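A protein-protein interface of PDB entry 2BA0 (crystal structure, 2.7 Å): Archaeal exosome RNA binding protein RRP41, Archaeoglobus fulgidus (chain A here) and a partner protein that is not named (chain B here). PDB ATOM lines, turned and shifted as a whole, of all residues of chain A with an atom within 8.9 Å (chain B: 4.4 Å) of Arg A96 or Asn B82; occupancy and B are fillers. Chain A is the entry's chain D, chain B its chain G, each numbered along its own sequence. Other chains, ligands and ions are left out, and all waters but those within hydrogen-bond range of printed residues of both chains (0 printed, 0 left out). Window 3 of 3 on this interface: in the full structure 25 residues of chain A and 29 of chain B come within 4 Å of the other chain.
NH1 of Arg A96 lies within hydrogen-bond range of O of Val B81. The guanidinium group (NH2) of Arg A96 sits close to the side-chain amide nitrogen (ND2) of Asn B82 (3.2 Å).
N of Asn B82 is in hydrogen-bond range of O of Val B137, at 3.0 Å. The backbone NH (N) of Ile B139 sits at hydrogen-bond distance from the backbone carbonyl oxygen (O) of Asn B82 (2.9 Å).
Of the 14 printed residues of chain A, 1 touches a printed residue of chain B. Of the 9 printed residues of chain B, 4 touch a printed residue of chain A. Hydrophobic or aromatic side chains of chain B within 4 Å of the printed part of chain A: Ile B103 and Ala B106.
Arg A96 touches Ile B103 (NH2 to CG1, 3.8 Å). Arg A96 touches Ala B106 (NH1 to CB, 3.9 Å).
Arg A96 touches just these residues of chain B: Val B81 (3.0 Å), Asn B82 (3.2 Å), Ile B103 (3.8 Å) and Ala B106 (3.9 Å). Of chain A, only Arg A96 comes within 4 Å of Asn B82. Printed residues of chain A within 4 Å of Val B81: Arg A96 (3.0 Å). Printed residues of chain A within 4 Å of Ala B106: Arg A96 (3.9 Å). Printed residues of chain A within 4 Å of Ile B103: Arg A96 (3.8 Å). Asp B138 touches none of the printed residues of chain A. The nearest printed residue of chain B that does not touch Arg A96 is Ala B83 (5.4 Å). The nearest printed residue of chain A that does not touch Asn B82 is Ile A99 (10.6 Å). The nearest printed residue of chain A that does not touch Ile B103 is Ile A99 (4.05 Å).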
ATOM      1  N   TYR A  79       6.228  -6.135  21.582  1.00  0.00           N
ATOM      2  CA  TYR A  79       5.053  -5.473  22.150  1.00  0.00           C
ATOM      3  C   TYR A  79       4.531  -6.396  23.235  1.00  0.00           C
ATOM      4  O   TYR A  79       4.369  -7.584  23.009  1.00  0.00           O
ATOM      5  CB  TYR A  79       3.990  -5.297  21.086  1.00  0.00           C
ATOM      6  CG  TYR A  79       2.678  -4.782  21.612  1.00  0.00           C
ATOM      7  CD1 TYR A  79       2.353  -3.422  21.529  1.00  0.00           C
ATOM      8  CD2 TYR A  79       1.715  -5.667  22.117  1.00  0.00           C
ATOM      9  CE1 TYR A  79       1.091  -2.953  21.921  1.00  0.00           C
ATOM     10  CE2 TYR A  79       0.452  -5.212  22.510  1.00  0.00           C
ATOM     11  CZ  TYR A  79       0.142  -3.859  22.399  1.00  0.00           C
ATOM     12  OH  TYR A  79      -1.138  -3.438  22.688  1.00  0.00           O
ATOM     13  N   LYS A  90      -4.704 -10.492  32.468  1.00  0.00           N
ATOM     14  CA  LYS A  90      -4.236 -11.249  31.329  1.00  0.00           C
ATOM     15  C   LYS A  90      -3.077 -12.165  31.680  1.00  0.00           C
ATOM     16  O   LYS A  90      -2.178 -11.805  32.423  1.00  0.00           O
ATOM     17  CB  LYS A  90      -3.829 -10.301  30.207  1.00  0.00           C
ATOM     18  CG  LYS A  90      -3.481 -11.023  28.928  1.00  0.00           C
ATOM     19  CD  LYS A  90      -3.145 -10.066  27.795  1.00  0.00           C
ATOM     20  CE  LYS A  90      -2.605 -10.849  26.605  1.00  0.00           C
ATOM     21  NZ  LYS A  90      -2.282  -9.979  25.450  1.00  0.00           N
ATOM     22  N   GLY A  93       2.697 -13.557  28.653  1.00  0.00           N
ATOM     23  CA  GLY A  93       3.141 -14.307  27.496  1.00  0.00           C
ATOM     24  C   GLY A  93       2.544 -13.776  26.205  1.00  0.00           C
ATOM     25  O   GLY A  93       1.501 -13.122  26.221  1.00  0.00           O
ATOM     26  N   PRO A  94       3.182 -14.046  25.060  1.00  0.00           N
ATOM     27  CA  PRO A  94       2.644 -13.549  23.796  1.00  0.00           C
ATOM     28  C   PRO A  94       1.406 -14.295  23.322  1.00  0.00           C
ATOM     29  O   PRO A  94       1.153 -15.432  23.712  1.00  0.00           O
ATOM     30  CB  PRO A  94       3.817 -13.722  22.839  1.00  0.00           C
ATOM     31  CG  PRO A  94       4.443 -14.987  23.334  1.00  0.00           C
ATOM     32  CD  PRO A  94       4.437 -14.791  24.839  1.00  0.00           C
ATOM     33  N   ASP A  95       0.636 -13.619  22.484  1.00  0.00           N
ATOM     34  CA  ASP A  95      -0.565 -14.175  21.892  1.00  0.00           C
ATOM     35  C   ASP A  95      -0.405 -13.861  20.407  1.00  0.00           C
ATOM     36  O   ASP A  95       0.555 -13.199  20.022  1.00  0.00           O
ATOM     37  CB  ASP A  95      -1.806 -13.493  22.466  1.00  0.00           C
ATOM     38  CG  ASP A  95      -1.638 -11.996  22.585  1.00  0.00           C
ATOM     39  OD1 ASP A  95      -0.862 -11.559  23.457  1.00  0.00           O
ATOM     40  OD2 ASP A  95      -2.269 -11.251  21.806  1.00  0.00           O
ATOM     41  N   ARG A  96      -1.322 -14.329  19.574  1.00  0.00           N
ATOM     42  CA  ARG A  96      -1.211 -14.083  18.146  1.00  0.00           C
ATOM     43  C   ARG A  96      -1.260 -12.582  17.855  1.00  0.00           C
ATOM     44  O   ARG A  96      -0.590 -12.091  16.940  1.00  0.00           O
ATOM     45  CB  ARG A  96      -2.324 -14.822  17.398  1.00  0.00           C
ATOM     46  CG  ARG A  96      -2.519 -16.249  17.883  1.00  0.00           C
ATOM     47  CD  ARG A  96      -2.373 -17.267  16.778  1.00  0.00           C
ATOM     48  NE  ARG A  96      -3.381 -17.116  15.738  1.00  0.00           N
ATOM     49  CZ  ARG A  96      -3.422 -17.856  14.632  1.00  0.00           C
ATOM     50  NH1 ARG A  96      -4.377 -17.659  13.723  1.00  0.00           N
ATOM     51  NH2 ARG A  96      -2.502 -18.796  14.433  1.00  0.00           N
ATOM     52  N   ARG A  97      -2.035 -11.851  18.647  1.00  0.00           N
ATOM     53  CA  ARG A  97      -2.154 -10.411  18.475  1.00  0.00           C
ATOM     54  C   ARG A  97      -0.829  -9.719  18.810  1.00  0.00           C
ATOM     55  O   ARG A  97      -0.333  -8.891  18.042  1.00  0.00           O
ATOM     56  CB  ARG A  97      -3.265  -9.883  19.374  1.00  0.00           C
ATOM     57  CG  ARG A  97      -3.564  -8.406  19.232  1.00  0.00           C
ATOM     58  CD  ARG A  97      -4.762  -8.022  20.083  1.00  0.00           C
ATOM     59  NE  ARG A  97      -5.022  -6.591  20.020  1.00  0.00           N
ATOM     60  CZ  ARG A  97      -4.407  -5.677  20.767  1.00  0.00           C
ATOM     61  NH1 ARG A  97      -4.720  -4.396  20.617  1.00  0.00           N
ATOM     62  NH2 ARG A  97      -3.501  -6.039  21.675  1.00  0.00           N
ATOM     63  N   SER A  98      -0.255 -10.059  19.956  1.00  0.00           N
ATOM     64  CA  SER A  98       1.013  -9.471  20.365  1.00  0.00           C
ATOM     65  C   SER A  98       2.067  -9.688  19.289  1.00  0.00           C
ATOM     66  O   SER A  98       2.825  -8.774  18.943  1.00  0.00           O
ATOM     67  CB  SER A  98       1.496 -10.095  21.681  1.00  0.00           C
ATOM     68  N   ILE A  99       2.112 -10.901  18.757  1.00  0.00           N
ATOM     69  CA  ILE A  99       3.083 -11.244  17.734  1.00  0.00           C
ATOM     70  C   ILE A  99       2.876 -10.434  16.453  1.00  0.00           C
ATOM     71  O   ILE A  99       3.844 -10.030  15.809  1.00  0.00           O
ATOM     72  CB  ILE A  99       3.032 -12.762  17.418  1.00  0.00           C
ATOM     73  CG1 ILE A  99       3.363 -13.561  18.683  1.00  0.00           C
ATOM     74  CG2 ILE A  99       4.037 -13.113  16.345  1.00  0.00           C
ATOM     75  CD1 ILE A  99       3.177 -15.057  18.534  1.00  0.00           C
ATOM     76  N   GLU A 100       1.626 -10.174  16.084  1.00  0.00           N
ATOM     77  CA  GLU A 100       1.385  -9.410  14.871  1.00  0.00           C
ATOM     78  C   GLU A 100       1.735  -7.939  15.068  1.00  0.00           C
ATOM     79  O   GLU A 100       2.293  -7.294  14.176  1.00  0.00           O
ATOM     80  CB  GLU A 100      -0.066  -9.553  14.421  1.00  0.00           C
ATOM     81  CG  GLU A 100      -0.212  -9.443  12.913  1.00  0.00           C
ATOM     82  CD  GLU A 100      -1.373  -8.558  12.497  1.00  0.00           C
ATOM     83  OE1 GLU A 100      -2.536  -9.047  12.449  1.00  0.00           O
ATOM     84  OE2 GLU A 100      -1.113  -7.357  12.227  1.00  0.00           O
ATOM     85  N   ILE A 101       1.413  -7.397  16.234  1.00  0.00           N
ATOM     86  CA  ILE A 101       1.740  -6.008  16.494  1.00  0.00           C
ATOM     87  C   ILE A 101       3.260  -5.846  16.479  1.00  0.00           C
ATOM     88  O   ILE A 101       3.786  -4.926  15.847  1.00  0.00           O
ATOM     89  CB  ILE A 101       1.168  -5.551  17.846  1.00  0.00           C
ATOM     90  CG1 ILE A 101      -0.346  -5.414  17.720  1.00  0.00           C
ATOM     91  CG2 ILE A 101       1.805  -4.233  18.288  1.00  0.00           C
ATOM     92  CD1 ILE A 101      -1.038  -5.101  19.025  1.00  0.00           C
ATOM     93  N   SER A 102       3.963  -6.751  17.155  1.00  0.00           N
ATOM     94  CA  SER A 102       5.413  -6.688  17.183  1.00  0.00           C
ATOM     95  C   SER A 102       6.013  -6.669  15.782  1.00  0.00           C
ATOM     96  O   SER A 102       6.942  -5.894  15.503  1.00  0.00           O
ATOM     97  CB  SER A 102       5.974  -7.872  17.960  1.00  0.00           C
ATOM     98  OG  SER A 102       5.610  -7.787  19.325  1.00  0.00           O
ATOM     99  N   LYS A 103       5.477  -7.516  14.906  1.00  0.00           N
ATOM    100  CA  LYS A 103       5.949  -7.624  13.525  1.00  0.00           C
ATOM    101  C   LYS A 103       5.782  -6.364  12.660  1.00  0.00           C
ATOM    102  O   LYS A 103       6.722  -5.900  12.008  1.00  0.00           O
ATOM    103  CB  LYS A 103       5.246  -8.779  12.823  1.00  0.00           C
ATOM    104  CG  LYS A 103       5.702  -8.932  11.393  1.00  0.00           C
ATOM    105  CD  LYS A 103       4.974 -10.048  10.692  1.00  0.00           C
ATOM    106  CE  LYS A 103       5.440 -10.173   9.260  1.00  0.00           C
ATOM    107  NZ  LYS A 103       4.597 -11.155   8.546  1.00  0.00           N
ATOM    108  N   ARG A 137      -1.146   0.309  20.575  1.00  0.00           N
ATOM    109  CA  ARG A 137      -0.268  -0.018  19.454  1.00  0.00           C
ATOM    110  C   ARG A 137       0.385   1.278  18.971  1.00  0.00           C
ATOM    111  O   ARG A 137       1.597   1.363  18.791  1.00  0.00           O
ATOM    112  CB  ARG A 137      -1.118  -0.623  18.338  1.00  0.00           C
ATOM    113  CG  ARG A 137      -0.423  -0.824  17.036  1.00  0.00           C
ATOM    114  CD  ARG A 137      -1.422  -1.253  15.984  1.00  0.00           C
ATOM    115  NE  ARG A 137      -2.342  -2.248  16.516  1.00  0.00           N
ATOM    116  CZ  ARG A 137      -2.905  -3.201  15.784  1.00  0.00           C
ATOM    117  NH1 ARG A 137      -3.736  -4.075  16.342  1.00  0.00           N
ATOM    118  NH2 ARG A 137      -2.624  -3.287  14.493  1.00  0.00           N
ATOM    119  N   ILE B  80     -12.775 -19.642  13.758  1.00  0.00           N
ATOM    120  CA  ILE B  80     -11.351 -19.679  14.063  1.00  0.00           C
ATOM    121  C   ILE B  80     -10.579 -20.010  12.798  1.00  0.00           C
ATOM    122  O   ILE B  80     -10.771 -21.077  12.221  1.00  0.00           O
ATOM    123  CB  ILE B  80     -11.027 -20.754  15.103  1.00  0.00           C
ATOM    124  CG1 ILE B  80     -11.799 -20.485  16.390  1.00  0.00           C
ATOM    125  CG2 ILE B  80      -9.550 -20.758  15.391  1.00  0.00           C
ATOM    126  CD1 ILE B  80     -11.580 -21.537  17.464  1.00  0.00           C
ATOM    127  N   VAL B  81      -9.710 -19.099  12.364  1.00  0.00           N
ATOM    128  CA  VAL B  81      -8.899 -19.318  11.163  1.00  0.00           C
ATOM    129  C   VAL B  81      -7.418 -19.548  11.512  1.00  0.00           C
ATOM    130  O   VAL B  81      -6.798 -18.762  12.248  1.00  0.00           O
ATOM    131  CB  VAL B  81      -9.018 -18.122  10.190  1.00  0.00           C
ATOM    132  CG1 VAL B  81      -8.157 -18.356   8.949  1.00  0.00           C
ATOM    133  CG2 VAL B  81     -10.465 -17.937   9.779  1.00  0.00           C
ATOM    134  N   ASN B  82      -6.859 -20.633  10.981  1.00  0.00           N
ATOM    135  CA  ASN B  82      -5.463 -20.991  11.225  1.00  0.00           C
ATOM    136  C   ASN B  82      -4.835 -21.498   9.927  1.00  0.00           C
ATOM    137  O   ASN B  82      -5.534 -22.042   9.074  1.00  0.00           O
ATOM    138  CB  ASN B  82      -5.391 -22.064  12.321  1.00  0.00           C
ATOM    139  CG  ASN B  82      -3.966 -22.348  12.787  1.00  0.00           C
ATOM    140  OD1 ASN B  82      -3.231 -23.128  12.168  1.00  0.00           O
ATOM    141  ND2 ASN B  82      -3.569 -21.709  13.883  1.00  0.00           N
ATOM    142  N   ALA B  83      -3.522 -21.320   9.773  1.00  0.00           N
ATOM    143  CA  ALA B  83      -2.837 -21.760   8.557  1.00  0.00           C
ATOM    144  C   ALA B  83      -1.549 -22.528   8.791  1.00  0.00           C
ATOM    145  O   ALA B  83      -0.818 -22.260   9.728  1.00  0.00           O
ATOM    146  CB  ALA B  83      -2.538 -20.574   7.675  1.00  0.00           C
ATOM    147  N   ILE B 103       1.009 -16.913  10.956  1.00  0.00           N
ATOM    148  CA  ILE B 103       0.044 -16.208  11.782  1.00  0.00           C
ATOM    149  C   ILE B 103      -0.543 -14.978  11.097  1.00  0.00           C
ATOM    150  O   ILE B 103      -1.736 -14.703  11.216  1.00  0.00           O
ATOM    151  CB  ILE B 103       0.687 -15.813  13.134  1.00  0.00           C
ATOM    152  CG1 ILE B 103       0.904 -17.081  13.971  1.00  0.00           C
ATOM    153  CG2 ILE B 103      -0.181 -14.777  13.872  1.00  0.00           C
ATOM    154  CD1 ILE B 103       1.347 -16.821  15.384  1.00  0.00           C
ATOM    155  N   ALA B 106      -3.019 -15.869   8.198  1.00  0.00           N
ATOM    156  CA  ALA B 106      -4.289 -16.307   8.744  1.00  0.00           C
ATOM    157  C   ALA B 106      -5.087 -15.105   9.247  1.00  0.00           C
ATOM    158  O   ALA B 106      -6.297 -15.021   9.026  1.00  0.00           O
ATOM    159  CB  ALA B 106      -4.055 -17.309   9.873  1.00  0.00           C
ATOM    160  N   VAL B 137     -11.539 -22.833  10.105  1.00  0.00           N
ATOM    161  CA  VAL B 137     -11.101 -22.655   8.723  1.00  0.00           C
ATOM    162  C   VAL B 137      -9.597 -22.908   8.738  1.00  0.00           C
ATOM    163  O   VAL B 137      -8.823 -22.084   9.227  1.00  0.00           O
ATOM    164  CB  VAL B 137     -11.418 -21.216   8.196  1.00  0.00           C
ATOM    165  CG1 VAL B 137     -10.929 -21.055   6.770  1.00  0.00           C
ATOM    166  CG2 VAL B 137     -12.905 -20.974   8.234  1.00  0.00           C
ATOM    167  N   ASP B 138      -9.196 -24.070   8.234  1.00  0.00           N
ATOM    168  CA  ASP B 138      -7.791 -24.450   8.206  1.00  0.00           C
ATOM    169  C   ASP B 138      -7.174 -24.375   6.815  1.00  0.00           C
ATOM    170  O   ASP B 138      -7.556 -25.112   5.902  1.00  0.00           O
ATOM    171  CB  ASP B 138      -7.618 -25.851   8.784  1.00  0.00           C
ATOM    172  CG  ASP B 138      -7.915 -25.901  10.274  1.00  0.00           C
ATOM    173  OD1 ASP B 138      -9.022 -26.344  10.657  1.00  0.00           O
ATOM    174  OD2 ASP B 138      -7.041 -25.485  11.070  1.00  0.00           O
ATOM    175  N   ILE B 139      -6.205 -23.469   6.680  1.00  0.00           N
ATOM    176  CA  ILE B 139      -5.500 -23.231   5.424  1.00  0.00           C
ATOM    177  C   ILE B 139      -4.252 -24.103   5.379  1.00  0.00           C
ATOM    178  O   ILE B 139      -3.475 -24.144   6.329  1.00  0.00           O
ATOM    179  CB  ILE B 139      -5.113 -21.744   5.315  1.00  0.00           C
ATOM    180  CG1 ILE B 139      -6.356 -20.885   5.549  1.00  0.00           C
ATOM    181  CG2 ILE B 139      -4.499 -21.450   3.946  1.00  0.00           C
ATOM    182  CD1 ILE B 139      -6.046 -19.434   5.735  1.00  0.00           C
